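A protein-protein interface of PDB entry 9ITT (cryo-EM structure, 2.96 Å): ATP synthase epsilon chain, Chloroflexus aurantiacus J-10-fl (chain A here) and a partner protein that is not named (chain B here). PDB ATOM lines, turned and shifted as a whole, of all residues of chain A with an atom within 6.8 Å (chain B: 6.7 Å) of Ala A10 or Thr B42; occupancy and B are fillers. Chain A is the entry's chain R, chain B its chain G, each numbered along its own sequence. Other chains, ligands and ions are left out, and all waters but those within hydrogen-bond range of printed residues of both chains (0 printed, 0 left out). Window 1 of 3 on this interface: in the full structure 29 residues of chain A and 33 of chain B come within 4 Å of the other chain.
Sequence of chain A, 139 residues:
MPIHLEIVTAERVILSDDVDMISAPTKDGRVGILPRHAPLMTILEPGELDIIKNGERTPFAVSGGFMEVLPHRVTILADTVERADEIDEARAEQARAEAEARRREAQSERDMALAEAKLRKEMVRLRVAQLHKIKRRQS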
ATOM      1  N   VAL A   8     -18.780  -7.476  21.406  1.00  0.00           N
ATOM      2  CA  VAL A   8     -18.962  -8.553  20.439  1.00  0.00           C
ATOM      3  C   VAL A   8     -19.636  -7.989  19.197  1.00  0.00           C
ATOM      4  O   VAL A   8     -20.736  -7.432  19.278  1.00  0.00           O
ATOM      5  CB  VAL A   8     -19.795  -9.708  21.023  1.00  0.00           C
ATOM      6  CG1 VAL A   8     -19.900 -10.848  20.018  1.00  0.00           C
ATOM      7  CG2 VAL A   8     -19.191 -10.190  22.325  1.00  0.00           C
ATOM      8  N   THR A   9     -18.972  -8.138  18.056  1.00  0.00           N
ATOM      9  CA  THR A   9     -19.548  -7.872  16.750  1.00  0.00           C
ATOM     10  C   THR A   9     -19.577  -9.179  15.971  1.00  0.00           C
ATOM     11  O   THR A   9     -18.784 -10.088  16.233  1.00  0.00           O
ATOM     12  CB  THR A   9     -18.741  -6.811  15.988  1.00  0.00           C
ATOM     13  OG1 THR A   9     -18.626  -5.631  16.791  1.00  0.00           O
ATOM     14  CG2 THR A   9     -19.415  -6.450  14.672  1.00  0.00           C
ATOM     15  N   ALA A  10     -20.510  -9.281  15.022  1.00  0.00           N
ATOM     16  CA  ALA A  10     -20.615 -10.505  14.237  1.00  0.00           C
ATOM     17  C   ALA A  10     -19.320 -10.800  13.493  1.00  0.00           C
ATOM     18  O   ALA A  10     -18.874 -11.951  13.460  1.00  0.00           O
ATOM     19  CB  ALA A  10     -21.780 -10.404  13.255  1.00  0.00           C
ATOM     20  N   GLU A  11     -18.694  -9.777  12.911  1.00  0.00           N
ATOM     21  CA  GLU A  11     -17.432  -9.987  12.211  1.00  0.00           C
ATOM     22  C   GLU A  11     -16.350 -10.502  13.153  1.00  0.00           C
ATOM     23  O   GLU A  11     -15.594 -11.412  12.798  1.00  0.00           O
ATOM     24  CB  GLU A  11     -16.982  -8.687  11.547  1.00  0.00           C
ATOM     25  CG  GLU A  11     -17.652  -8.410  10.214  1.00  0.00           C
ATOM     26  CD  GLU A  11     -19.109  -8.014  10.360  1.00  0.00           C
ATOM     27  OE1 GLU A  11     -19.644  -8.110  11.484  1.00  0.00           O
ATOM     28  OE2 GLU A  11     -19.717  -7.606   9.348  1.00  0.00           O
ATOM     29  N   ARG A  12     -16.256  -9.934  14.353  1.00  0.00           N
ATOM     30  CA  ARG A  12     -15.207 -10.327  15.283  1.00  0.00           C
ATOM     31  C   ARG A  12     -15.556  -9.831  16.676  1.00  0.00           C
ATOM     32  O   ARG A  12     -16.437  -8.987  16.854  1.00  0.00           O
ATOM     33  CB  ARG A  12     -13.845  -9.776  14.847  1.00  0.00           C
ATOM     34  CG  ARG A  12     -13.777  -8.254  14.794  1.00  0.00           C
ATOM     35  CD  ARG A  12     -12.425  -7.776  14.299  1.00  0.00           C
ATOM     36  NE  ARG A  12     -11.354  -8.106  15.232  1.00  0.00           N
ATOM     37  CZ  ARG A  12     -10.059  -8.050  14.947  1.00  0.00           C
ATOM     38  NH1 ARG A  12      -9.624  -7.671  13.756  1.00  0.00           N
ATOM     39  NH2 ARG A  12      -9.175  -8.382  15.883  1.00  0.00           N
ATOM     40  N   VAL A  13     -14.844 -10.369  17.662  1.00  0.00           N
ATOM     41  CA  VAL A  13     -14.910  -9.889  19.037  1.00  0.00           C
ATOM     42  C   VAL A  13     -13.754  -8.913  19.225  1.00  0.00           C
ATOM     43  O   VAL A  13     -12.587  -9.308  19.183  1.00  0.00           O
ATOM     44  CB  VAL A  13     -14.834 -11.044  20.042  1.00  0.00           C
ATOM     45  CG1 VAL A  13     -15.027 -10.529  21.463  1.00  0.00           C
ATOM     46  CG2 VAL A  13     -15.868 -12.109  19.704  1.00  0.00           C
ATOM     47  N   ILE A  14     -14.077  -7.639  19.438  1.00  0.00           N
ATOM     48  CA  ILE A  14     -13.041  -6.613  19.491  1.00  0.00           C
ATOM     49  C   ILE A  14     -12.386  -6.578  20.866  1.00  0.00           C
ATOM     50  O   ILE A  14     -11.155  -6.533  20.977  1.00  0.00           O
ATOM     51  CB  ILE A  14     -13.626  -5.241  19.102  1.00  0.00           C
ATOM     52  CG1 ILE A  14     -14.272  -5.316  17.715  1.00  0.00           C
ATOM     53  CG2 ILE A  14     -12.536  -4.168  19.116  1.00  0.00           C
ATOM     54  CD1 ILE A  14     -15.769  -5.533  17.733  1.00  0.00           C
ATOM     55  N   LEU A  77     -23.939  -6.953  22.110  1.00  0.00           N
ATOM     56  CA  LEU A  77     -23.995  -7.558  20.782  1.00  0.00           C
ATOM     57  C   LEU A  77     -24.275  -6.414  19.818  1.00  0.00           C
ATOM     58  O   LEU A  77     -25.422  -6.145  19.459  1.00  0.00           O
ATOM     59  CB  LEU A  77     -25.064  -8.649  20.719  1.00  0.00           C
ATOM     60  CG  LEU A  77     -24.938  -9.745  21.784  1.00  0.00           C
ATOM     61  CD1 LEU A  77     -26.186 -10.611  21.810  1.00  0.00           C
ATOM     62  CD2 LEU A  77     -23.702 -10.603  21.568  1.00  0.00           C
ATOM     63  N   ALA A  78     -23.210  -5.740  19.402  1.00  0.00           N
ATOM     64  CA  ALA A  78     -23.300  -4.503  18.645  1.00  0.00           C
ATOM     65  C   ALA A  78     -23.122  -4.762  17.157  1.00  0.00           C
ATOM     66  O   ALA A  78     -22.213  -5.480  16.733  1.00  0.00           O
ATOM     67  CB  ALA A  78     -22.247  -3.506  19.127  1.00  0.00           C
ATOM     68  N   ASP A  79     -24.011  -4.165  16.362  1.00  0.00           N
ATOM     69  CA  ASP A  79     -23.960  -4.353  14.916  1.00  0.00           C
ATOM     70  C   ASP A  79     -22.670  -3.788  14.332  1.00  0.00           C
ATOM     71  O   ASP A  79     -22.060  -4.397  13.446  1.00  0.00           O
ATOM     72  CB  ASP A  79     -25.179  -3.705  14.260  1.00  0.00           C
ATOM     73  CG  ASP A  79     -25.313  -2.233  14.599  1.00  0.00           C
ATOM     74  OD1 ASP A  79     -24.534  -1.745  15.444  1.00  0.00           O
ATOM     75  OD2 ASP A  79     -26.195  -1.566  14.020  1.00  0.00           O
ATOM     76  N   ARG B  37     -11.401 -20.039  10.243  1.00  0.00           N
ATOM     77  CA  ARG B  37     -11.059 -19.007  11.215  1.00  0.00           C
ATOM     78  C   ARG B  37     -12.174 -17.975  11.326  1.00  0.00           C
ATOM     79  O   ARG B  37     -12.532 -17.552  12.432  1.00  0.00           O
ATOM     80  CB  ARG B  37      -9.745 -18.333  10.828  1.00  0.00           C
ATOM     81  CG  ARG B  37      -8.523 -18.945  11.482  1.00  0.00           C
ATOM     82  CD  ARG B  37      -7.246 -18.322  10.949  1.00  0.00           C
ATOM     83  NE  ARG B  37      -6.946 -18.771   9.595  1.00  0.00           N
ATOM     84  CZ  ARG B  37      -5.841 -18.467   8.925  1.00  0.00           C
ATOM     85  NH1 ARG B  37      -4.899 -17.701   9.451  1.00  0.00           N
ATOM     86  NH2 ARG B  37      -5.679 -18.944   7.694  1.00  0.00           N
ATOM     87  N   ASN B  38     -12.739 -17.562  10.191  1.00  0.00           N
ATOM     88  CA  ASN B  38     -13.834 -16.597  10.215  1.00  0.00           C
ATOM     89  C   ASN B  38     -15.065 -17.170  10.906  1.00  0.00           C
ATOM     90  O   ASN B  38     -15.741 -16.465  11.663  1.00  0.00           O
ATOM     91  CB  ASN B  38     -14.177 -16.163   8.793  1.00  0.00           C
ATOM     92  CG  ASN B  38     -13.230 -15.111   8.264  1.00  0.00           C
ATOM     93  OD1 ASN B  38     -12.160 -14.885   8.828  1.00  0.00           O
ATOM     94  ND2 ASN B  38     -13.615 -14.463   7.175  1.00  0.00           N
ATOM     95  N   VAL B  39     -15.379 -18.439  10.650  1.00  0.00           N
ATOM     96  CA  VAL B  39     -16.528 -19.061  11.305  1.00  0.00           C
ATOM     97  C   VAL B  39     -16.326 -19.082  12.815  1.00  0.00           C
ATOM     98  O   VAL B  39     -17.238 -18.751  13.586  1.00  0.00           O
ATOM     99  CB  VAL B  39     -16.762 -20.476  10.743  1.00  0.00           C
ATOM    100  CG1 VAL B  39     -17.693 -21.277  11.647  1.00  0.00           C
ATOM    101  CG2 VAL B  39     -17.329 -20.399   9.338  1.00  0.00           C
ATOM    102  N   LEU B  40     -15.131 -19.467  13.262  1.00  0.00           N
ATOM    103  CA  LEU B  40     -14.872 -19.504  14.697  1.00  0.00           C
ATOM    104  C   LEU B  40     -14.869 -18.108  15.306  1.00  0.00           C
ATOM    105  O   LEU B  40     -15.256 -17.942  16.467  1.00  0.00           O
ATOM    106  CB  LEU B  40     -13.548 -20.215  14.979  1.00  0.00           C
ATOM    107  CG  LEU B  40     -13.610 -21.731  15.205  1.00  0.00           C
ATOM    108  CD1 LEU B  40     -14.378 -22.070  16.477  1.00  0.00           C
ATOM    109  CD2 LEU B  40     -14.220 -22.457  14.013  1.00  0.00           C
ATOM    110  N   ALA B  41     -14.437 -17.098  14.550  1.00  0.00           N
ATOM    111  CA  ALA B  41     -14.470 -15.729  15.052  1.00  0.00           C
ATOM    112  C   ALA B  41     -15.887 -15.173  15.101  1.00  0.00           C
ATOM    113  O   ALA B  41     -16.164 -14.263  15.888  1.00  0.00           O
ATOM    114  CB  ALA B  41     -13.588 -14.830  14.185  1.00  0.00           C
ATOM    115  N   THR B  42     -16.780 -15.683  14.252  1.00  0.00           N
ATOM    116  CA  THR B  42     -18.183 -15.286  14.298  1.00  0.00           C
ATOM    117  C   THR B  42     -18.956 -16.062  15.360  1.00  0.00           C
ATOM    118  O   THR B  42     -20.016 -15.607  15.804  1.00  0.00           O
ATOM    119  CB  THR B  42     -18.815 -15.493  12.918  1.00  0.00           C
ATOM    120  OG1 THR B  42     -17.969 -14.905  11.923  1.00  0.00           O
ATOM    121  CG2 THR B  42     -20.202 -14.853  12.818  1.00  0.00           C
ATOM    122  N   ARG B  43     -18.441 -17.217  15.777  1.00  0.00           N
ATOM    123  CA  ARG B  43     -19.136 -18.050  16.758  1.00  0.00           C
ATOM    124  C   ARG B  43     -19.550 -17.327  18.039  1.00  0.00           C
ATOM    125  O   ARG B  43     -20.664 -17.595  18.525  1.00  0.00           O
ATOM    126  CB  ARG B  43     -18.246 -19.255  17.102  1.00  0.00           C
ATOM    127  CG  ARG B  43     -18.884 -20.316  18.000  1.00  0.00           C
ATOM    128  CD  ARG B  43     -20.080 -21.001  17.354  1.00  0.00           C
ATOM    129  NE  ARG B  43     -19.686 -21.792  16.192  1.00  0.00           N
ATOM    130  CZ  ARG B  43     -20.346 -22.844  15.724  1.00  0.00           C
ATOM    131  NH1 ARG B  43     -21.468 -23.270  16.285  1.00  0.00           N
ATOM    132  NH2 ARG B  43     -19.869 -23.486  14.661  1.00  0.00           N
ATOM    133  N   PRO B  44     -18.729 -16.466  18.656  1.00  0.00           N
ATOM    134  CA  PRO B  44     -19.159 -15.842  19.920  1.00  0.00           C
ATOM    135  C   PRO B  44     -20.431 -15.025  19.798  1.00  0.00           C
ATOM    136  O   PRO B  44     -21.322 -15.168  20.642  1.00  0.00           O
ATOM    137  CB  PRO B  44     -17.960 -14.961  20.301  1.00  0.00           C
ATOM    138  CG  PRO B  44     -16.808 -15.570  19.593  1.00  0.00           C
ATOM    139  CD  PRO B  44     -17.370 -16.037  18.293  1.00  0.00           C
ATOM    140  N   TYR B  45     -20.541 -14.164  18.786  1.00  0.00           N
ATOM    141  CA  TYR B  45     -21.788 -13.439  18.572  1.00  0.00           C
ATOM    142  C   TYR B  45     -22.963 -14.399  18.453  1.00  0.00           C
ATOM    143  O   TYR B  45     -23.993 -14.211  19.118  1.00  0.00           O
ATOM    144  CB  TYR B  45     -21.664 -12.574  17.315  1.00  0.00           C
ATOM    145  CG  TYR B  45     -22.745 -11.531  17.128  1.00  0.00           C
ATOM    146  CD1 TYR B  45     -24.033 -11.890  16.759  1.00  0.00           C
ATOM    147  CD2 TYR B  45     -22.470 -10.184  17.303  1.00  0.00           C
ATOM    148  CE1 TYR B  45     -25.016 -10.940  16.580  1.00  0.00           C
ATOM    149  CE2 TYR B  45     -23.447  -9.226  17.127  1.00  0.00           C
ATOM    150  CZ  TYR B  45     -24.718  -9.610  16.766  1.00  0.00           C
ATOM    151  OH  TYR B  45     -25.697  -8.660  16.588  1.00  0.00           O
ATOM    152  N   ALA B  46     -22.804 -15.450  17.647  1.00  0.00           N
ATOM    153  CA  ALA B  46     -23.901 -16.374  17.395  1.00  0.00           C
ATOM    154  C   ALA B  46     -24.368 -17.043  18.680  1.00  0.00           C
ATOM    155  O   ALA B  46     -25.562 -17.028  18.994  1.00  0.00           O
ATOM    156  CB  ALA B  46     -23.473 -17.424  16.371  1.00  0.00           C
ATOM    157  N   ASP B  47     -23.447 -17.621  19.452  1.00  0.00           N
ATOM    158  CA  ASP B  47     -23.886 -18.362  20.629  1.00  0.00           C
ATOM    159  C   ASP B  47     -24.347 -17.444  21.759  1.00  0.00           C
ATOM    160  O   ASP B  47     -25.314 -17.784  22.458  1.00  0.00           O
ATOM    161  CB  ASP B  47     -22.783 -19.322  21.108  1.00  0.00           C
ATOM    162  CG  ASP B  47     -21.654 -18.631  21.860  1.00  0.00           C
ATOM    163  OD1 ASP B  47     -21.519 -17.399  21.786  1.00  0.00           O
ATOM    164  OD2 ASP B  47     -20.885 -19.344  22.538  1.00  0.00           O
ATOM    165  N   LEU B 149     -21.607  -8.962   7.279  1.00  0.00           N
ATOM    166  CA  LEU B 149     -23.040  -9.088   7.516  1.00  0.00           C
ATOM    167  C   LEU B 149     -23.833  -8.013   6.790  1.00  0.00           C
ATOM    168  O   LEU B 149     -24.988  -8.254   6.423  1.00  0.00           O
ATOM    169  CB  LEU B 149     -23.337  -9.033   9.015  1.00  0.00           C
ATOM    170  CG  LEU B 149     -24.767  -9.413   9.416  1.00  0.00           C
ATOM    171  CD1 LEU B 149     -24.760 -10.223  10.701  1.00  0.00           C
ATOM    172  CD2 LEU B 149     -25.647  -8.182   9.582  1.00  0.00           C
ATOM    173  N   ARG B 223     -32.443  -9.425  14.230  1.00  0.00           N
ATOM    174  CA  ARG B 223     -30.993  -9.563  14.303  1.00  0.00           C
ATOM    175  C   ARG B 223     -30.592 -11.008  14.561  1.00  0.00           C
ATOM    176  O   ARG B 223     -29.570 -11.471  14.049  1.00  0.00           O
ATOM    177  CB  ARG B 223     -30.426  -8.644  15.384  1.00  0.00           C
ATOM    178  CG  ARG B 223     -28.909  -8.474  15.330  1.00  0.00           C
ATOM    179  CD  ARG B 223     -28.464  -7.638  14.136  1.00  0.00           C
ATOM    180  NE  ARG B 223     -27.013  -7.601  14.001  1.00  0.00           N
ATOM    181  CZ  ARG B 223     -26.362  -6.952  13.044  1.00  0.00           C
ATOM    182  NH1 ARG B 223     -27.002  -6.259  12.115  1.00  0.00           N
ATOM    183  NH2 ARG B 223     -25.034  -7.000  13.018  1.00  0.00           N
ATOM    184  N   THR B 227     -28.243 -13.131  12.141  1.00  0.00           N
ATOM    185  CA  THR B 227     -27.085 -13.866  12.636  1.00  0.00           C
ATOM    186  C   THR B 227     -27.118 -15.316  12.178  1.00  0.00           C
ATOM    187  O   THR B 227     -26.085 -15.877  11.797  1.00  0.00           O
ATOM    188  CB  THR B 227     -27.031 -13.793  14.161  1.00  0.00           C
ATOM    189  OG1 THR B 227     -27.097 -12.425  14.581  1.00  0.00           O
ATOM    190  CG2 THR B 227     -25.752 -14.426  14.685  1.00  0.00           C
ATOM    191  N   TYR B 230     -26.124 -15.358   8.564  1.00  0.00           N
ATOM    192  CA  TYR B 230     -24.690 -15.118   8.423  1.00  0.00           C
ATOM    193  C   TYR B 230     -23.890 -16.363   8.783  1.00  0.00           C
ATOM    194  O   TYR B 230     -22.915 -16.706   8.099  1.00  0.00           O
ATOM    195  CB  TYR B 230     -24.283 -13.939   9.307  1.00  0.00           C
ATOM    196  CG  TYR B 230     -22.887 -13.401   9.075  1.00  0.00           C
ATOM    197  CD1 TYR B 230     -22.452 -13.054   7.807  1.00  0.00           C
ATOM    198  CD2 TYR B 230     -22.016 -13.215  10.137  1.00  0.00           C
ATOM    199  CE1 TYR B 230     -21.184 -12.555   7.598  1.00  0.00           C
ATOM    200  CE2 TYR B 230     -20.747 -12.715   9.939  1.00  0.00           C
ATOM    201  CZ  TYR B 230     -20.337 -12.386   8.667  1.00  0.00           C
ATOM    202  OH  TYR B 230     -19.072 -11.888   8.466  1.00  0.00           O
ATOM    203  N   GLN B 231     -24.285 -17.050   9.857  1.00  0.00           N
ATOM    204  CA  GLN B 231     -23.644 -18.312  10.207  1.00  0.00           C
ATOM    205  C   GLN B 231     -23.772 -19.316   9.074  1.00  0.00           C
ATOM    206  O   GLN B 231     -22.798 -19.990   8.718  1.00  0.00           O
ATOM    207  CB  GLN B 231     -24.265 -18.879  11.483  1.00  0.00           C
ATOM    208  CG  GLN B 231     -23.893 -18.144  12.754  1.00  0.00           C
ATOM    209  CD  GLN B 231     -22.435 -18.310  13.114  1.00  0.00           C
ATOM    210  OE1 GLN B 231     -21.655 -17.365  13.043  1.00  0.00           O
ATOM    211  NE2 GLN B 231     -22.058 -19.520  13.507  1.00  0.00           N
ATOM    212  N   LEU B 234     -21.408 -18.306   6.140  1.00  0.00           N
ATOM    213  CA  LEU B 234     -20.003 -18.605   6.402  1.00  0.00           C
ATOM    214  C   LEU B 234     -19.751 -20.108   6.393  1.00  0.00           C
ATOM    215  O   LEU B 234     -18.719 -20.571   5.887  1.00  0.00           O
ATOM    216  CB  LEU B 234     -19.576 -17.990   7.732  1.00  0.00           C
ATOM    217  CG  LEU B 234     -19.611 -16.462   7.786  1.00  0.00           C
ATOM    218  CD1 LEU B 234     -19.409 -15.996   9.212  1.00  0.00           C
ATOM    219  CD2 LEU B 234     -18.569 -15.848   6.863  1.00  0.00           C
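Of the 17 printed residues of chain B, 5 touch a printed residue of chain A.
Hydrophobic or aromatic side chains of chain B within 4 Å of the printed part of chain A: Pro B44, Tyr B45 and Leu B149.
Along chain B the printed residues that touch a printed residue of chain A span positions 42 to 223.
Hydrophobic or aromatic side chains of chain A within 4 Å of the printed part of chain B: Val A8, Ala A10, Val A13 and Leu A77.
Among the printed residues, 10 pairs touch across the chains.
The backbone carbonyl oxygen (O) of Pro B44 sits close to the side-chain carboxylate (OD1) of Asp B47, at 2.5 Å.
OH of Tyr B45 sits at hydrogen-bond distance from NE of Arg B223, at 3.1 Å.
O of Val A8 lies within hydrogen-bond range of N of Ala A78 (3.0 Å).
The side-chain hydroxyl (OG1) of Thr B42 lies within hydrogen-bond range of the backbone carbonyl oxygen (O) of Asn B38, 2.7 Å away.
O of Arg B223 lies within hydrogen-bond range of OG1 of Thr B227 (2.7 Å).
The backbone carbonyl oxygen (O) of Ala A10 lies close to the side-chain hydroxyl (OG1) of Thr B42.
The backbone NH of Leu B149 lies within hydrogen-bond range of the side-chain carboxylate of Glu A11, at 3.1 Å.
Among the printed residues, pairs that only touch across the chains: Val A8 with Tyr B45 (3.5 Å), Thr A9 with Tyr B45 (3.3 Å), Ala A10 with Tyr B45 (3.1 Å), Ala A10 with Leu B149 (3.9 Å), Val A13 with Pro B44 (3.6 Å), Leu A77 with Tyr B45 (3.8 Å), Ala A78 with Tyr B45 (3.96 Å) and Asp A79 with Arg B223 (3.4 Å).
Printed residues of chain B within 4 Å of Val A8: Tyr B45.
Ala A10 touches three residues of chain B.
Printed residues of chain B within 4 Å of Leu A77: Tyr B45.
Ala B41 touches none of the printed residues of chain A.
Thr B42 touches one residue of chain A.
Printed residues of chain A within 4 Å of Pro B44: Val A13.
The nearest residue of chain B that does not touch Ala A10 is Tyr B230 (4.1 Å).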
